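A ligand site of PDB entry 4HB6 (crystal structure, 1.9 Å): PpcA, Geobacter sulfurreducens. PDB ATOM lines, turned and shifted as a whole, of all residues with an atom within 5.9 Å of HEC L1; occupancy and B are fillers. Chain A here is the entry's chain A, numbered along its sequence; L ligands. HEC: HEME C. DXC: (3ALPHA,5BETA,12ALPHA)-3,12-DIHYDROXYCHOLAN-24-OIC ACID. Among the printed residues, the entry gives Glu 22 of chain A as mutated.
The backbone carbonyl oxygen of Asp 2 lies close to an oxygen (O1D) of HEC L1. Residues that only touch HEC L1: Asp 3 (3.5 Å), Ile 4 (3.96 Å), Phe 15 (3.6 Å), His 20 (3.7 Å), Gln 21 (3.4 Å), Val 24 (3.4 Å) and Pro 25 (3.997 Å). Hydrophobic or aromatic side chains that line HEC L1: Ala 1, Phe 15, His 17, His 20, Val 24 and His 31. The nearest printed residue that does not touch HEC L1 is Asp 26 (4.6 Å).
ND1 of His 20 is in hydrogen-bond range of O of Pro 16. N of His 17 sits at hydrogen-bond distance from OD1 of Asp 3 (3.0 Å). N of Phe 15 is in hydrogen-bond range of O of Ile 4, 3.0 Å away. A ring nitrogen (ND1) of His 17 lies close to the side-chain amide nitrogen of Gln 21, 3.4 Å away.
NE2 of His 17 is bound to FE of HEC L1 (2.0 Å). The side-chain sulfur of Cys 27 is bonded to a carbon (CAB) of HEC L1. O2A of HEC L1 is in hydrogen-bond range of N of Ala 1 (2.7 Å). SG of Cys 30 is bonded to CAC of HEC L1 (2.0 Å). An iron atom (FE) of HEC L1 is bound by a ring nitrogen (NE2) of His 31 (2.0 Å). NE2 of His 20 is bound to FE of HEC L2.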
ATOM      1  N   ALA A   1       1.241  13.823 -21.552  1.00  0.00           N
ATOM      2  CA  ALA A   1       1.986  13.875 -20.267  1.00  0.00           C
ATOM      3  C   ALA A   1       1.063  14.266 -19.144  1.00  0.00           C
ATOM      4  O   ALA A   1      -0.011  14.809 -19.368  1.00  0.00           O
ATOM      5  CB  ALA A   1       3.137  14.870 -20.355  1.00  0.00           C
ATOM      6  N   ASP A   2       1.518  14.026 -17.931  1.00  0.00           N
ATOM      7  CA  ASP A   2       0.763  14.346 -16.741  1.00  0.00           C
ATOM      8  C   ASP A   2       1.099  15.709 -16.168  1.00  0.00           C
ATOM      9  O   ASP A   2       2.191  16.228 -16.409  1.00  0.00           O
ATOM     10  CB  ASP A   2       1.050  13.284 -15.710  1.00  0.00           C
ATOM     11  CG  ASP A   2       0.489  11.956 -16.106  1.00  0.00           C
ATOM     12  OD1 ASP A   2      -0.727  11.937 -16.449  1.00  0.00           O
ATOM     13  OD2 ASP A   2       1.197  10.907 -16.133  1.00  0.00           O
ATOM     14  N   ASP A   3       0.159  16.295 -15.429  1.00  0.00           N
ATOM     15  CA  ASP A   3       0.454  17.475 -14.626  1.00  0.00           C
ATOM     16  C   ASP A   3       1.464  17.106 -13.548  1.00  0.00           C
ATOM     17  O   ASP A   3       1.677  15.944 -13.258  1.00  0.00           O
ATOM     18  CB  ASP A   3      -0.803  18.069 -14.015  1.00  0.00           C
ATOM     19  CG  ASP A   3      -1.696  18.736 -15.055  1.00  0.00           C
ATOM     20  OD1 ASP A   3      -1.216  19.019 -16.162  1.00  0.00           O
ATOM     21  OD2 ASP A   3      -2.877  18.997 -14.837  1.00  0.00           O
ATOM     22  N   ILE A   4       2.135  18.107 -13.030  1.00  0.00           N
ATOM     23  CA  ILE A   4       3.077  17.879 -11.976  1.00  0.00           C
ATOM     24  C   ILE A   4       2.689  18.669 -10.742  1.00  0.00           C
ATOM     25  O   ILE A   4       1.938  19.643 -10.821  1.00  0.00           O
ATOM     26  CB  ILE A   4       4.499  18.197 -12.422  1.00  0.00           C
ATOM     27  CG1 ILE A   4       4.628  19.652 -12.755  1.00  0.00           C
ATOM     28  CG2 ILE A   4       4.848  17.362 -13.633  1.00  0.00           C
ATOM     29  CD1 ILE A   4       6.007  19.986 -13.158  1.00  0.00           C
ATOM     30  N   PHE A  15       0.298  22.101 -10.705  1.00  0.00           N
ATOM     31  CA  PHE A  15       0.478  22.893 -11.901  1.00  0.00           C
ATOM     32  C   PHE A  15      -0.328  22.260 -13.024  1.00  0.00           C
ATOM     33  O   PHE A  15       0.106  21.252 -13.579  1.00  0.00           O
ATOM     34  CB  PHE A  15       1.939  22.969 -12.331  1.00  0.00           C
ATOM     35  CG  PHE A  15       2.105  23.672 -13.636  1.00  0.00           C
ATOM     36  CD1 PHE A  15       2.045  25.055 -13.697  1.00  0.00           C
ATOM     37  CD2 PHE A  15       2.252  22.960 -14.826  1.00  0.00           C
ATOM     38  CE1 PHE A  15       2.190  25.725 -14.897  1.00  0.00           C
ATOM     39  CE2 PHE A  15       2.383  23.615 -16.036  1.00  0.00           C
ATOM     40  CZ  PHE A  15       2.356  25.008 -16.073  1.00  0.00           C
ATOM     41  N   PRO A  16      -1.498  22.828 -13.328  1.00  0.00           N
ATOM     42  CA  PRO A  16      -2.354  22.278 -14.391  1.00  0.00           C
ATOM     43  C   PRO A  16      -1.991  22.833 -15.776  1.00  0.00           C
ATOM     44  O   PRO A  16      -2.198  24.017 -16.059  1.00  0.00           O
ATOM     45  CB  PRO A  16      -3.761  22.692 -13.935  1.00  0.00           C
ATOM     46  CG  PRO A  16      -3.549  23.985 -13.203  1.00  0.00           C
ATOM     47  CD  PRO A  16      -2.154  23.939 -12.618  1.00  0.00           C
ATOM     48  N   HIS A  17      -1.465  21.967 -16.629  1.00  0.00           N
ATOM     49  CA  HIS A  17      -0.937  22.441 -17.915  1.00  0.00           C
ATOM     50  C   HIS A  17      -2.024  22.950 -18.854  1.00  0.00           C
ATOM     51  O   HIS A  17      -1.854  23.996 -19.479  1.00  0.00           O
ATOM     52  CB  HIS A  17      -0.110  21.382 -18.672  1.00  0.00           C
ATOM     53  CG  HIS A  17       0.585  21.958 -19.880  1.00  0.00           C
ATOM     54  ND1 HIS A  17       0.109  21.771 -21.156  1.00  0.00           N
ATOM     55  CD2 HIS A  17       1.624  22.809 -19.991  1.00  0.00           C
ATOM     56  CE1 HIS A  17       0.883  22.418 -22.017  1.00  0.00           C
ATOM     57  NE2 HIS A  17       1.822  23.061 -21.327  1.00  0.00           N
ATOM     58  N   HIS A  20      -3.030  26.482 -18.606  1.00  0.00           N
ATOM     59  CA  HIS A  20      -1.945  27.379 -19.036  1.00  0.00           C
ATOM     60  C   HIS A  20      -1.799  27.479 -20.558  1.00  0.00           C
ATOM     61  O   HIS A  20      -1.584  28.552 -21.100  1.00  0.00           O
ATOM     62  CB  HIS A  20      -0.656  26.970 -18.363  1.00  0.00           C
ATOM     63  CG  HIS A  20      -0.627  27.349 -16.907  1.00  0.00           C
ATOM     64  ND1 HIS A  20      -1.169  26.552 -15.926  1.00  0.00           N
ATOM     65  CD2 HIS A  20      -0.171  28.459 -16.284  1.00  0.00           C
ATOM     66  CE1 HIS A  20      -1.027  27.138 -14.756  1.00  0.00           C
ATOM     67  NE2 HIS A  20      -0.427  28.310 -14.943  1.00  0.00           N
ATOM     68  N   GLN A  21      -1.927  26.344 -21.233  1.00  0.00           N
ATOM     69  CA  GLN A  21      -1.877  26.301 -22.683  1.00  0.00           C
ATOM     70  C   GLN A  21      -3.020  27.135 -23.275  1.00  0.00           C
ATOM     71  O   GLN A  21      -2.851  27.872 -24.248  1.00  0.00           O
ATOM     72  CB  GLN A  21      -1.952  24.844 -23.132  1.00  0.00           C
ATOM     73  CG  GLN A  21      -1.682  24.616 -24.581  1.00  0.00           C
ATOM     74  CD  GLN A  21      -1.515  23.142 -24.920  1.00  0.00           C
ATOM     75  OE1 GLN A  21      -1.163  22.823 -26.044  1.00  0.00           O
ATOM     76  NE2 GLN A  21      -1.766  22.260 -23.975  1.00  0.00           N
ATOM     77  N   GLU A  22      -4.190  27.066 -22.631  1.00  0.00           N
ATOM     78  CA  GLU A  22      -5.366  27.853 -23.035  1.00  0.00           C
ATOM     79  C   GLU A  22      -5.282  29.369 -22.750  1.00  0.00           C
ATOM     80  O   GLU A  22      -5.597  30.175 -23.639  1.00  0.00           O
ATOM     81  CB  GLU A  22      -6.630  27.262 -22.397  1.00  0.00           C
ATOM     82  CG  GLU A  22      -7.026  25.944 -23.047  1.00  0.00           C
ATOM     83  CD  GLU A  22      -8.202  25.233 -22.376  1.00  0.00           C
ATOM     84  OE1 GLU A  22      -8.481  24.061 -22.738  1.00  0.00           O
ATOM     85  OE2 GLU A  22      -8.862  25.835 -21.497  1.00  0.00           O
ATOM     86  N   VAL A  24      -2.446  31.107 -21.824  1.00  0.00           N
ATOM     87  CA  VAL A  24      -1.156  31.693 -22.150  1.00  0.00           C
ATOM     88  C   VAL A  24      -0.695  31.212 -23.539  1.00  0.00           C
ATOM     89  O   VAL A  24       0.246  30.439 -23.683  1.00  0.00           O
ATOM     90  CB  VAL A  24      -0.068  31.401 -21.064  1.00  0.00           C
ATOM     91  CG1 VAL A  24       1.180  32.161 -21.344  1.00  0.00           C
ATOM     92  CG2 VAL A  24      -0.570  31.766 -19.692  1.00  0.00           C
ATOM     93  N   PRO A  25      -1.389  31.703 -24.572  1.00  0.00           N
ATOM     94  CA  PRO A  25      -1.055  31.325 -25.965  1.00  0.00           C
ATOM     95  C   PRO A  25       0.370  31.683 -26.387  1.00  0.00           C
ATOM     96  O   PRO A  25       0.928  31.056 -27.307  1.00  0.00           O
ATOM     97  CB  PRO A  25      -2.106  32.088 -26.799  1.00  0.00           C
ATOM     98  CG  PRO A  25      -2.622  33.159 -25.918  1.00  0.00           C
ATOM     99  CD  PRO A  25      -2.512  32.649 -24.494  1.00  0.00           C
ATOM    100  N   ASP A  26       0.971  32.659 -25.731  1.00  0.00           N
ATOM    101  CA  ASP A  26       2.386  32.934 -25.884  1.00  0.00           C
ATOM    102  C   ASP A  26       3.193  31.846 -25.143  1.00  0.00           C
ATOM    103  O   ASP A  26       3.676  32.050 -24.023  1.00  0.00           O
ATOM    104  CB  ASP A  26       2.747  34.342 -25.387  1.00  0.00           C
ATOM    105  CG  ASP A  26       4.191  34.727 -25.688  1.00  0.00           C
ATOM    106  OD1 ASP A  26       4.859  34.019 -26.476  1.00  0.00           O
ATOM    107  OD2 ASP A  26       4.765  35.701 -25.138  1.00  0.00           O
ATOM    108  N   CYS A  27       3.389  30.722 -25.835  1.00  0.00           N
ATOM    109  CA  CYS A  27       4.071  29.542 -25.280  1.00  0.00           C
ATOM    110  C   CYS A  27       5.511  29.833 -24.900  1.00  0.00           C
ATOM    111  O   CYS A  27       6.036  29.197 -23.989  1.00  0.00           O
ATOM    112  CB  CYS A  27       4.032  28.366 -26.273  1.00  0.00           C
ATOM    113  SG  CYS A  27       2.448  28.055 -27.091  1.00  0.00           S
ATOM    114  N   LYS A  29       6.579  32.105 -23.241  1.00  0.00           N
ATOM    115  CA  LYS A  29       6.649  32.512 -21.825  1.00  0.00           C
ATOM    116  C   LYS A  29       7.296  31.448 -20.967  1.00  0.00           C
ATOM    117  O   LYS A  29       7.960  31.764 -20.005  1.00  0.00           O
ATOM    118  CB  LYS A  29       5.260  32.866 -21.294  1.00  0.00           C
ATOM    119  CG  LYS A  29       4.857  34.264 -21.703  1.00  0.00           C
ATOM    120  CD  LYS A  29       5.769  35.280 -21.020  1.00  0.00           C
ATOM    121  CE  LYS A  29       5.319  36.704 -21.194  1.00  0.00           C
ATOM    122  NZ  LYS A  29       6.053  37.564 -20.222  1.00  0.00           N
ATOM    123  N   CYS A  30       7.101  30.189 -21.323  1.00  0.00           N
ATOM    124  CA  CYS A  30       7.684  29.087 -20.570  1.00  0.00           C
ATOM    125  C   CYS A  30       8.544  28.138 -21.351  1.00  0.00           C
ATOM    126  O   CYS A  30       9.400  27.470 -20.757  1.00  0.00           O
ATOM    127  CB  CYS A  30       6.548  28.276 -19.979  1.00  0.00           C
ATOM    128  SG  CYS A  30       5.561  29.251 -18.851  1.00  0.00           S
ATOM    129  N   HIS A  31       8.278  28.008 -22.647  1.00  0.00           N
ATOM    130  CA  HIS A  31       8.996  27.059 -23.490  1.00  0.00           C
ATOM    131  C   HIS A  31      10.059  27.723 -24.374  1.00  0.00           C
ATOM    132  O   HIS A  31      10.025  28.917 -24.613  1.00  0.00           O
ATOM    133  CB  HIS A  31       8.016  26.268 -24.344  1.00  0.00           C
ATOM    134  CG  HIS A  31       7.088  25.405 -23.560  1.00  0.00           C
ATOM    135  ND1 HIS A  31       7.541  24.426 -22.693  1.00  0.00           N
ATOM    136  CD2 HIS A  31       5.735  25.366 -23.490  1.00  0.00           C
ATOM    137  CE1 HIS A  31       6.496  23.822 -22.134  1.00  0.00           C
ATOM    138  NE2 HIS A  31       5.392  24.376 -22.601  1.00  0.00           N
ATOM    139  N   GLY A  50       8.004  33.246 -12.077  1.00  0.00           N
ATOM    140  CA  GLY A  50       7.777  31.848 -12.362  1.00  0.00           C
ATOM    141  C   GLY A  50       6.348  31.372 -12.218  1.00  0.00           C
ATOM    142  O   GLY A  50       5.904  30.462 -12.925  1.00  0.00           O
HETATM  143 FE   HEC L   1       3.599  23.726 -22.007  1.00  0.00          FE
HETATM  144  CHA HEC L   1       4.247  20.506 -21.089  1.00  0.00           C
HETATM  145  CHB HEC L   1       3.282  22.753 -25.257  1.00  0.00           C
HETATM  146  CHC HEC L   1       2.190  26.760 -22.696  1.00  0.00           C
HETATM  147  CHD HEC L   1       4.775  24.868 -19.065  1.00  0.00           C
HETATM  148  NA  HEC L   1       3.812  22.016 -22.976  1.00  0.00           N
HETATM  149  C1A HEC L   1       3.950  20.781 -22.407  1.00  0.00           C
HETATM  150  C2A HEC L   1       3.725  19.767 -23.403  1.00  0.00           C
HETATM  151  C3A HEC L   1       3.461  20.371 -24.548  1.00  0.00           C
HETATM  152  C4A HEC L   1       3.526  21.790 -24.330  1.00  0.00           C
HETATM  153  CMA HEC L   1       3.181  19.679 -25.903  1.00  0.00           C
HETATM  154  CAA HEC L   1       3.690  18.257 -23.130  1.00  0.00           C
HETATM  155  CBA HEC L   1       2.178  18.013 -22.852  1.00  0.00           C
HETATM  156  CGA HEC L   1       1.665  16.587 -22.927  1.00  0.00           C
HETATM  157  O1A HEC L   1       2.320  15.722 -23.578  1.00  0.00           O
HETATM  158  O2A HEC L   1       0.567  16.282 -22.345  1.00  0.00           O
HETATM  159  NB  HEC L   1       2.846  24.606 -23.679  1.00  0.00           N
HETATM  160  C1B HEC L   1       2.802  24.018 -24.927  1.00  0.00           C
HETATM  161  C2B HEC L   1       2.235  24.984 -25.848  1.00  0.00           C
HETATM  162  C3B HEC L   1       1.938  26.098 -25.149  1.00  0.00           C
HETATM  163  C4B HEC L   1       2.303  25.869 -23.757  1.00  0.00           C
HETATM  164  CMB HEC L   1       2.029  24.686 -27.363  1.00  0.00           C
HETATM  165  CAB HEC L   1       1.263  27.401 -25.652  1.00  0.00           C
HETATM  166  CBB HEC L   1      -0.011  27.385 -26.035  1.00  0.00           C
HETATM  167  NC  HEC L   1       3.476  25.456 -21.071  1.00  0.00           N
HETATM  168  C1C HEC L   1       2.870  26.631 -21.511  1.00  0.00           C
HETATM  169  C2C HEC L   1       3.097  27.658 -20.528  1.00  0.00           C
HETATM  170  C3C HEC L   1       3.797  27.117 -19.537  1.00  0.00           C
HETATM  171  C4C HEC L   1       4.061  25.744 -19.859  1.00  0.00           C
HETATM  172  CMC HEC L   1       2.606  29.111 -20.621  1.00  0.00           C
HETATM  173  CAC HEC L   1       4.288  27.834 -18.258  1.00  0.00           C
HETATM  174  CBC HEC L   1       3.356  28.526 -17.525  1.00  0.00           C
HETATM  175  ND  HEC L   1       4.417  22.835 -20.346  1.00  0.00           N
HETATM  176  C1D HEC L   1       4.825  23.519 -19.237  1.00  0.00           C
HETATM  177  C2D HEC L   1       5.282  22.567 -18.251  1.00  0.00           C
HETATM  178  C3D HEC L   1       5.095  21.193 -18.862  1.00  0.00           C
HETATM  179  C4D HEC L   1       4.561  21.468 -20.174  1.00  0.00           C
HETATM  180  CMD HEC L   1       5.821  22.864 -16.863  1.00  0.00           C
HETATM  181  CAD HEC L   1       5.408  19.821 -18.225  1.00  0.00           C
HETATM  182  CBD HEC L   1       4.481  19.599 -17.038  1.00  0.00           C
HETATM  183  CGD HEC L   1       3.028  19.452 -17.415  1.00  0.00           C
HETATM  184  O1D HEC L   1       2.718  18.926 -18.506  1.00  0.00           O
HETATM  185  O2D HEC L   1       2.202  19.865 -16.578  1.00  0.00           O
HETATM  186 FE   HEC L   2      -0.594  29.822 -13.647  1.00  0.00          FE
HETATM  187  CHA HEC L   2      -3.972  29.656 -13.751  1.00  0.00           C
HETATM  188  CHB HEC L   2      -0.620  27.628 -10.992  1.00  0.00           C
HETATM  189  CHC HEC L   2       2.811  29.686 -13.631  1.00  0.00           C
HETATM  190  CHD HEC L   2      -0.506  32.145 -16.081  1.00  0.00           C
HETATM  191  NA  HEC L   2      -2.014  28.813 -12.570  1.00  0.00           N
HETATM  192  C1A HEC L   2      -3.366  28.880 -12.805  1.00  0.00           C
HETATM  193  C2A HEC L   2      -4.053  27.973 -11.908  1.00  0.00           C
HETATM  194  C3A HEC L   2      -3.136  27.403 -11.137  1.00  0.00           C
HETATM  195  C4A HEC L   2      -1.835  27.920 -11.532  1.00  0.00           C
HETATM  196  CMA HEC L   2      -3.405  26.372 -10.015  1.00  0.00           C
HETATM  197  CAA HEC L   2      -5.586  27.760 -11.833  1.00  0.00           C
HETATM  198  CBA HEC L   2      -6.111  27.065 -13.069  1.00  0.00           C
HETATM  199  CGA HEC L   2      -7.615  26.951 -13.039  1.00  0.00           C
HETATM  200  O1A HEC L   2      -8.303  27.763 -12.363  1.00  0.00           O
HETATM  201  O2A HEC L   2      -8.114  26.027 -13.710  1.00  0.00           O
HETATM  202  NB  HEC L   2       0.823  28.846 -12.531  1.00  0.00           N
HETATM  203  C1B HEC L   2       0.608  28.015 -11.487  1.00  0.00           C
HETATM  204  C2B HEC L   2       1.860  27.598 -10.951  1.00  0.00           C
HETATM  205  C3B HEC L   2       2.818  28.129 -11.705  1.00  0.00           C
HETATM  206  C4B HEC L   2       2.163  28.940 -12.705  1.00  0.00           C
HETATM  207  CMB HEC L   2       2.022  26.654  -9.753  1.00  0.00           C
HETATM  208  CAB HEC L   2       4.316  27.966 -11.546  1.00  0.00           C
HETATM  209  CBB HEC L   2       4.793  26.702 -11.354  1.00  0.00           C
HETATM  210  NC  HEC L   2       0.888  30.754 -14.661  1.00  0.00           N
HETATM  211  C1C HEC L   2       2.223  30.558 -14.509  1.00  0.00           C
HETATM  212  C2C HEC L   2       2.915  31.404 -15.437  1.00  0.00           C
HETATM  213  C3C HEC L   2       2.003  32.084 -16.143  1.00  0.00           C
HETATM  214  C4C HEC L   2       0.711  31.676 -15.653  1.00  0.00           C
HETATM  215  CMC HEC L   2       4.455  31.464 -15.566  1.00  0.00           C
HETATM  216  CAC HEC L   2       2.219  33.112 -17.292  1.00  0.00           C
HETATM  217  CBC HEC L   2       3.402  33.255 -17.927  1.00  0.00           C
HETATM  218  ND  HEC L   2      -1.978  30.722 -14.746  1.00  0.00           N
HETATM  219  C1D HEC L   2      -1.731  31.738 -15.663  1.00  0.00           C
HETATM  220  C2D HEC L   2      -2.970  32.302 -16.130  1.00  0.00           C
HETATM  221  C3D HEC L   2      -4.051  31.523 -15.423  1.00  0.00           C
HETATM  222  C4D HEC L   2      -3.351  30.562 -14.586  1.00  0.00           C
HETATM  223  CMD HEC L   2      -3.195  33.459 -17.138  1.00  0.00           C
HETATM  224  CAD HEC L   2      -5.574  31.712 -15.559  1.00  0.00           C
HETATM  225  CBD HEC L   2      -6.125  30.468 -16.224  1.00  0.00           C
HETATM  226  CGD HEC L   2      -7.628  30.383 -16.106  1.00  0.00           C
HETATM  227  O1D HEC L   2      -8.203  30.673 -15.018  1.00  0.00           O
HETATM  228  O2D HEC L   2      -8.254  30.028 -17.128  1.00  0.00           O
HETATM  229  C1  DXC L   3      11.150  22.370 -11.267  1.00  0.00           C
HETATM  230  C2  DXC L   3       9.709  22.906 -11.369  1.00  0.00           C
HETATM  231  C3  DXC L   3       9.055  22.486 -12.701  1.00  0.00           C
HETATM  232  C4  DXC L   3       9.869  22.851 -13.949  1.00  0.00           C
HETATM  233  C5  DXC L   3      11.315  22.326 -13.777  1.00  0.00           C
HETATM  234  C6  DXC L   3      11.932  22.855 -12.488  1.00  0.00           C
HETATM  235  C7  DXC L   3       7.615  23.050 -12.767  1.00  0.00           C
HETATM  236  C8  DXC L   3       7.614  24.598 -13.032  1.00  0.00           C
HETATM  237  C9  DXC L   3       8.424  24.924 -14.304  1.00  0.00           C
HETATM  238  C10 DXC L   3       9.860  24.364 -14.209  1.00  0.00           C
HETATM  239  C11 DXC L   3       8.529  26.434 -14.516  1.00  0.00           C
HETATM  240  C12 DXC L   3       9.250  26.839 -15.804  1.00  0.00           C
HETATM  241  C13 DXC L   3      10.674  26.304 -15.736  1.00  0.00           C
HETATM  242  C14 DXC L   3      10.677  24.784 -15.476  1.00  0.00           C
HETATM  243  C15 DXC L   3       7.169  27.161 -14.629  1.00  0.00           C
HETATM  244  C16 DXC L   3       7.536  28.446 -15.380  1.00  0.00           C
HETATM  245  C17 DXC L   3       9.026  28.365 -15.718  1.00  0.00           C
HETATM  246  C18 DXC L   3       9.265  22.081 -15.133  1.00  0.00           C
HETATM  247  C19 DXC L   3       9.316  29.199 -16.987  1.00  0.00           C
HETATM  248  O1  DXC L   3      11.401  26.916 -14.661  1.00  0.00           O
HETATM  249  O2  DXC L   3      11.787  22.875 -10.116  1.00  0.00           O
HETATM  250  C20 DXC L   3       8.561  26.255 -17.042  1.00  0.00           C
HETATM  251  C21 DXC L   3       8.833  30.649 -16.883  1.00  0.00           C
HETATM  252  C22 DXC L   3       9.541  31.411 -15.776  1.00  0.00           C
HETATM  253  C23 DXC L   3      10.751  32.192 -16.280  1.00  0.00           C
HETATM  254  O3  DXC L   3      10.623  33.079 -17.126  1.00  0.00           O
HETATM  255  O4  DXC L   3      11.869  31.940 -15.812  1.00  0.00           O
HETATM  256  C24 DXC L   3      10.788  29.136 -17.392  1.00  0.00           C
